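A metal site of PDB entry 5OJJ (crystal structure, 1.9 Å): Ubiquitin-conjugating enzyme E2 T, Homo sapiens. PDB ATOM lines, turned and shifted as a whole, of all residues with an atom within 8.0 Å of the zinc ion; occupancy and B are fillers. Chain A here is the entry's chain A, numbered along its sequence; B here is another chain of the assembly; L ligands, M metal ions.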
ATOM      1  N   ASN A  78      16.519  -0.141   2.456  1.00  0.00           N
ATOM      2  CA  ASN A  78      16.999  -1.519   2.520  1.00  0.00           C
ATOM      3  C   ASN A  78      17.911  -1.959   1.362  1.00  0.00           C
ATOM      4  O   ASN A  78      18.221  -3.143   1.245  1.00  0.00           O
ATOM      5  CB  ASN A  78      15.800  -2.504   2.595  1.00  0.00           C
ATOM      6  CG  ASN A  78      14.743  -2.083   3.631  1.00  0.00           C
ATOM      7  OD1 ASN A  78      13.558  -1.999   3.308  1.00  0.00           O
ATOM      8  ND2 ASN A  78      15.177  -1.774   4.840  1.00  0.00           N
ATOM      9  N   ARG A  84      23.149  -4.091  -2.806  1.00  0.00           N
ATOM     10  CA  ARG A  84      22.860  -5.172  -1.882  1.00  0.00           C
ATOM     11  C   ARG A  84      21.500  -4.937  -1.244  1.00  0.00           C
ATOM     12  O   ARG A  84      21.116  -3.777  -1.034  1.00  0.00           O
ATOM     13  CB  ARG A  84      23.922  -5.288  -0.784  1.00  0.00           C
ATOM     14  CG  ARG A  84      25.296  -5.648  -1.306  1.00  0.00           C
ATOM     15  CD  ARG A  84      26.348  -5.752  -0.214  1.00  0.00           C
ATOM     16  NE  ARG A  84      26.731  -4.446   0.343  1.00  0.00           N
ATOM     17  CZ  ARG A  84      27.794  -4.189   1.104  1.00  0.00           C
ATOM     18  NH1 ARG A  84      28.663  -5.145   1.420  1.00  0.00           N
ATOM     19  NH2 ARG A  84      28.005  -2.958   1.531  1.00  0.00           N
ATOM     20  N   ILE A  85      20.818  -6.038  -0.907  1.00  0.00           N
ATOM     21  CA  ILE A  85      19.389  -6.005  -0.515  1.00  0.00           C
ATOM     22  C   ILE A  85      19.174  -6.696   0.827  1.00  0.00           C
ATOM     23  O   ILE A  85      19.499  -7.881   0.952  1.00  0.00           O
ATOM     24  CB  ILE A  85      18.504  -6.729  -1.569  1.00  0.00           C
ATOM     25  CG1 ILE A  85      18.698  -6.154  -2.975  1.00  0.00           C
ATOM     26  CG2 ILE A  85      17.025  -6.714  -1.139  1.00  0.00           C
ATOM     27  CD1 ILE A  85      18.169  -7.022  -4.085  1.00  0.00           C
ATOM     28  N   CYS A  86      18.622  -5.986   1.812  1.00  0.00           N
ATOM     29  CA  CYS A  86      18.324  -6.604   3.129  1.00  0.00           C
ATOM     30  C   CYS A  86      16.899  -7.149   3.119  1.00  0.00           C
ATOM     31  O   CYS A  86      15.928  -6.399   3.178  1.00  0.00           O
ATOM     32  CB  CYS A  86      18.519  -5.630   4.307  1.00  0.00           C
ATOM     33  SG  CYS A  86      18.421  -6.442   5.934  1.00  0.00           S
ATOM     34  N   LEU A  87      16.789  -8.485   3.034  1.00  0.00           N
ATOM     35  CA  LEU A  87      15.486  -9.155   2.887  1.00  0.00           C
ATOM     36  C   LEU A  87      15.568 -10.545   3.488  1.00  0.00           C
ATOM     37  O   LEU A  87      16.553 -11.250   3.265  1.00  0.00           O
ATOM     38  CB  LEU A  87      15.111  -9.219   1.399  1.00  0.00           C
ATOM     39  CG  LEU A  87      13.732  -9.814   1.047  1.00  0.00           C
ATOM     40  CD1 LEU A  87      12.602  -9.037   1.680  1.00  0.00           C
ATOM     41  CD2 LEU A  87      13.519  -9.900  -0.460  1.00  0.00           C
ATOM     42  N   ASP A  88      14.545 -10.934   4.280  1.00  0.00           N
ATOM     43  CA  ASP A  88      14.568 -12.212   5.026  1.00  0.00           C
ATOM     44  C   ASP A  88      14.793 -13.443   4.156  1.00  0.00           C
ATOM     45  O   ASP A  88      15.588 -14.299   4.520  1.00  0.00           O
ATOM     46  CB  ASP A  88      13.305 -12.424   5.911  1.00  0.00           C
ATOM     47  CG  ASP A  88      11.975 -12.410   5.129  1.00  0.00           C
ATOM     48  OD1 ASP A  88      11.911 -12.174   3.901  1.00  0.00           O
ATOM     49  OD2 ASP A  88      10.930 -12.639   5.794  1.00  0.00           O
ATOM     50  N   LEU A  90      16.503 -13.798   1.543  1.00  0.00           N
ATOM     51  CA  LEU A  90      17.854 -13.826   1.058  1.00  0.00           C
ATOM     52  C   LEU A  90      18.882 -14.184   2.123  1.00  0.00           C
ATOM     53  O   LEU A  90      20.094 -14.151   1.844  1.00  0.00           O
ATOM     54  CB  LEU A  90      18.210 -12.486   0.390  1.00  0.00           C
ATOM     55  CG  LEU A  90      17.330 -12.083  -0.802  1.00  0.00           C
ATOM     56  CD1 LEU A  90      17.776 -10.733  -1.362  1.00  0.00           C
ATOM     57  CD2 LEU A  90      17.314 -13.129  -1.923  1.00  0.00           C
ATOM     58  N   LYS A  91      18.404 -14.548   3.332  1.00  0.00           N
ATOM     59  CA  LYS A  91      19.280 -14.863   4.459  1.00  0.00           C
ATOM     60  C   LYS A  91      19.074 -16.311   4.931  1.00  0.00           C
ATOM     61  O   LYS A  91      17.974 -16.846   4.789  1.00  0.00           O
ATOM     62  CB  LYS A  91      19.049 -13.897   5.614  1.00  0.00           C
ATOM     63  CG  LYS A  91      19.263 -12.423   5.274  1.00  0.00           C
ATOM     64  CD  LYS A  91      18.941 -11.561   6.478  1.00  0.00           C
ATOM     65  CE  LYS A  91      18.948 -10.063   6.231  1.00  0.00           C
ATOM     66  NZ  LYS A  91      20.343  -9.618   6.113  1.00  0.00           N
ATOM     67  N   LYS A  95      17.973 -17.406  11.602  1.00  0.00           N
ATOM     68  CA  LYS A  95      17.617 -15.978  11.547  1.00  0.00           C
ATOM     69  C   LYS A  95      16.802 -15.647  10.284  1.00  0.00           C
ATOM     70  O   LYS A  95      15.785 -14.970  10.372  1.00  0.00           O
ATOM     71  CB  LYS A  95      18.875 -15.106  11.643  1.00  0.00           C
ATOM     72  CG  LYS A  95      18.701 -13.573  11.547  1.00  0.00           C
ATOM     73  CD  LYS A  95      18.214 -13.095  10.173  1.00  0.00           C
ATOM     74  CE  LYS A  95      18.763 -11.754   9.739  1.00  0.00           C
ATOM     75  NZ  LYS A  95      18.167 -10.523  10.284  1.00  0.00           N
ATOM     76  N   ASP A 122      15.463  -2.332   9.081  1.00  0.00           N
ATOM     77  CA  ASP A 122      16.493  -3.116   8.379  1.00  0.00           C
ATOM     78  C   ASP A 122      17.411  -2.225   7.512  1.00  0.00           C
ATOM     79  O   ASP A 122      17.521  -2.447   6.297  1.00  0.00           O
ATOM     80  CB  ASP A 122      15.807  -4.155   7.450  1.00  0.00           C
ATOM     81  CG  ASP A 122      14.988  -5.211   8.180  1.00  0.00           C
ATOM     82  OD1 ASP A 122      15.065  -5.366   9.427  1.00  0.00           O
ATOM     83  OD2 ASP A 122      14.281  -5.940   7.463  1.00  0.00           O
ATOM     84  N   PRO A 123      18.126  -1.237   8.102  1.00  0.00           N
ATOM     85  CA  PRO A 123      18.834  -0.281   7.227  1.00  0.00           C
ATOM     86  C   PRO A 123      20.128  -0.792   6.577  1.00  0.00           C
ATOM     87  O   PRO A 123      20.957  -1.419   7.249  1.00  0.00           O
ATOM     88  CB  PRO A 123      19.160   0.868   8.191  1.00  0.00           C
ATOM     89  CG  PRO A 123      19.346   0.182   9.511  1.00  0.00           C
ATOM     90  CD  PRO A 123      18.298  -0.903   9.532  1.00  0.00           C
ATOM     91  N   LEU A 124      20.299  -0.499   5.289  1.00  0.00           N
ATOM     92  CA  LEU A 124      21.624  -0.552   4.634  1.00  0.00           C
ATOM     93  C   LEU A 124      22.177   0.831   4.233  1.00  0.00           C
ATOM     94  O   LEU A 124      23.340   0.918   3.839  1.00  0.00           O
ATOM     95  CB  LEU A 124      21.594  -1.467   3.409  1.00  0.00           C
ATOM     96  CG  LEU A 124      21.467  -2.985   3.636  1.00  0.00           C
ATOM     97  CD1 LEU A 124      21.435  -3.686   2.285  1.00  0.00           C
ATOM     98  CD2 LEU A 124      22.597  -3.518   4.506  1.00  0.00           C
ATOM     99  N   THR B  72      29.646  -8.948   3.084  1.00  0.00           N
ATOM    100  CA  THR B  72      28.701  -8.727   4.204  1.00  0.00           C
ATOM    101  C   THR B  72      28.722  -7.247   4.590  1.00  0.00           C
ATOM    102  O   THR B  72      29.805  -6.703   4.777  1.00  0.00           O
ATOM    103  CB  THR B  72      29.156  -9.529   5.451  1.00  0.00           C
ATOM    104  OG1 THR B  72      29.248 -10.914   5.124  1.00  0.00           O
ATOM    105  CG2 THR B  72      28.215  -9.339   6.629  1.00  0.00           C
ATOM    106  N   PRO B  73      27.540  -6.593   4.704  1.00  0.00           N
ATOM    107  CA  PRO B  73      27.531  -5.216   5.207  1.00  0.00           C
ATOM    108  C   PRO B  73      28.109  -5.084   6.607  1.00  0.00           C
ATOM    109  O   PRO B  73      27.976  -5.996   7.408  1.00  0.00           O
ATOM    110  CB  PRO B  73      26.025  -4.843   5.230  1.00  0.00           C
ATOM    111  CG  PRO B  73      25.363  -5.793   4.323  1.00  0.00           C
ATOM    112  CD  PRO B  73      26.186  -7.053   4.324  1.00  0.00           C
ATOM    113  N   TRP B 146      23.663  -3.307  13.327  1.00  0.00           N
ATOM    114  CA  TRP B 146      24.039  -3.758  11.971  1.00  0.00           C
ATOM    115  C   TRP B 146      24.649  -5.170  11.994  1.00  0.00           C
ATOM    116  O   TRP B 146      24.402  -5.985  11.106  1.00  0.00           O
ATOM    117  CB  TRP B 146      24.986  -2.761  11.262  1.00  0.00           C
ATOM    118  CG  TRP B 146      24.290  -1.556  10.680  1.00  0.00           C
ATOM    119  CD1 TRP B 146      23.415  -0.728  11.320  1.00  0.00           C
ATOM    120  CD2 TRP B 146      24.418  -1.031   9.348  1.00  0.00           C
ATOM    121  NE1 TRP B 146      22.973   0.259  10.479  1.00  0.00           N
ATOM    122  CE2 TRP B 146      23.572   0.099   9.259  1.00  0.00           C
ATOM    123  CE3 TRP B 146      25.154  -1.408   8.204  1.00  0.00           C
ATOM    124  CZ2 TRP B 146      23.460   0.870   8.096  1.00  0.00           C
ATOM    125  CZ3 TRP B 146      25.022  -0.664   7.065  1.00  0.00           C
ATOM    126  CH2 TRP B 146      24.195   0.468   7.013  1.00  0.00           C
ATOM    127  N   GLU B 148      23.909  -7.563  14.253  1.00  0.00           N
ATOM    128  CA  GLU B 148      22.730  -8.407  14.475  1.00  0.00           C
ATOM    129  C   GLU B 148      21.910  -8.593  13.199  1.00  0.00           C
ATOM    130  O   GLU B 148      21.511  -9.709  12.864  1.00  0.00           O
ATOM    131  CB  GLU B 148      21.853  -7.808  15.591  1.00  0.00           C
ATOM    132  CG  GLU B 148      20.793  -8.747  16.164  1.00  0.00           C
ATOM    133  CD  GLU B 148      19.523  -8.877  15.310  1.00  0.00           C
ATOM    134  OE1 GLU B 148      18.983  -7.844  14.850  1.00  0.00           O
ATOM    135  OE2 GLU B 148      19.058 -10.025  15.103  1.00  0.00           O
ATOM    136  N   LYS B 149      21.678  -7.495  12.473  1.00  0.00           N
ATOM    137  CA  LYS B 149      20.822  -7.533  11.272  1.00  0.00           C
ATOM    138  C   LYS B 149      21.417  -8.276  10.075  1.00  0.00           C
ATOM    139  O   LYS B 149      20.728  -9.107   9.453  1.00  0.00           O
ATOM    140  CB  LYS B 149      20.437  -6.116  10.862  1.00  0.00           C
ATOM    141  CG  LYS B 149      19.349  -6.019   9.793  1.00  0.00           C
ATOM    142  CD  LYS B 149      18.037  -6.650  10.209  1.00  0.00           C
ATOM    143  CE  LYS B 149      17.587  -6.096  11.555  1.00  0.00           C
ATOM    144  NZ  LYS B 149      16.139  -6.295  11.753  1.00  0.00           N
ATOM    145  N   HIS B 150      22.678  -7.989   9.757  1.00  0.00           N
ATOM    146  CA  HIS B 150      23.308  -8.401   8.494  1.00  0.00           C
ATOM    147  C   HIS B 150      24.391  -9.490   8.581  1.00  0.00           C
ATOM    148  O   HIS B 150      24.699 -10.126   7.577  1.00  0.00           O
ATOM    149  CB  HIS B 150      23.933  -7.180   7.812  1.00  0.00           C
ATOM    150  CG  HIS B 150      23.023  -6.006   7.768  1.00  0.00           C
ATOM    151  ND1 HIS B 150      21.744  -6.073   7.245  1.00  0.00           N
ATOM    152  CD2 HIS B 150      23.195  -4.723   8.169  1.00  0.00           C
ATOM    153  CE1 HIS B 150      21.171  -4.890   7.329  1.00  0.00           C
ATOM    154  NE2 HIS B 150      22.032  -4.048   7.889  1.00  0.00           N
ATOM    155  N   ALA B 151      24.998  -9.659   9.748  1.00  0.00           N
ATOM    156  CA  ALA B 151      26.044 -10.658   9.918  1.00  0.00           C
ATOM    157  C   ALA B 151      25.472 -11.805  10.766  1.00  0.00           C
ATOM    158  O   ALA B 151      25.150 -12.864  10.229  1.00  0.00           O
ATOM    159  CB  ALA B 151      27.281 -10.042  10.554  1.00  0.00           C
HETATM  160  C1  LIG L   1      22.340  -7.840   3.801  1.00  0.00           C
HETATM  161  O1  LIG L   1      21.348  -7.177   4.138  1.00  0.00           O
HETATM  162  O2  LIG L   1      22.902  -8.577   4.630  1.00  0.00           O
HETATM  163  C2  LIG L   1      22.877  -7.745   2.396  1.00  0.00           C
HETATM  164 ZN    ZN M   1      20.524  -7.433   5.957  1.00  0.00          ZN
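O1 of the ligand is bound to the zinc ion, at 2.0 Å.
The zinc ion is bound by NZ of Lys 91 (2.2 Å).
The zinc ion is bound by ND1 of His 150 of chain B (2.2 Å).
The side-chain sulfur (SG) of Cys 86 binds the zinc ion (2.3 Å).
The zinc ion has four donor atoms within binding distance.
Residues that only touch the zinc ion: Lys 149 of chain B.
Within 4 Å of the zinc ion: Cys 86, Lys 91, Lys 149 of chain B and His 150 of chain B.
The nearest printed residue that does not touch the zinc ion is Leu 124 (4.7 Å).
The side-chain amino group of Lys 91 sits close to the backbone carbonyl oxygen of Lys 149 of chain B.
O of Pro 123 lies within hydrogen-bond range of NE2 of His 150 of chain B (2.9 Å).
The backbone carbonyl oxygen (O) of Asn 78 lies within hydrogen-bond range of the backbone NH (N) of Cys 86, 2.9 Å away.
The backbone carbonyl oxygen (O) of Lys 149 of chain B is in hydrogen-bond range of the side-chain amino group (NZ) of Lys 95 (3.0 Å).
The side-chain carboxylate (OD1) of Asp 122 is in salt-bridge range of the side-chain amino group (NZ) of Lys 149 of chain B (2.7 Å).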
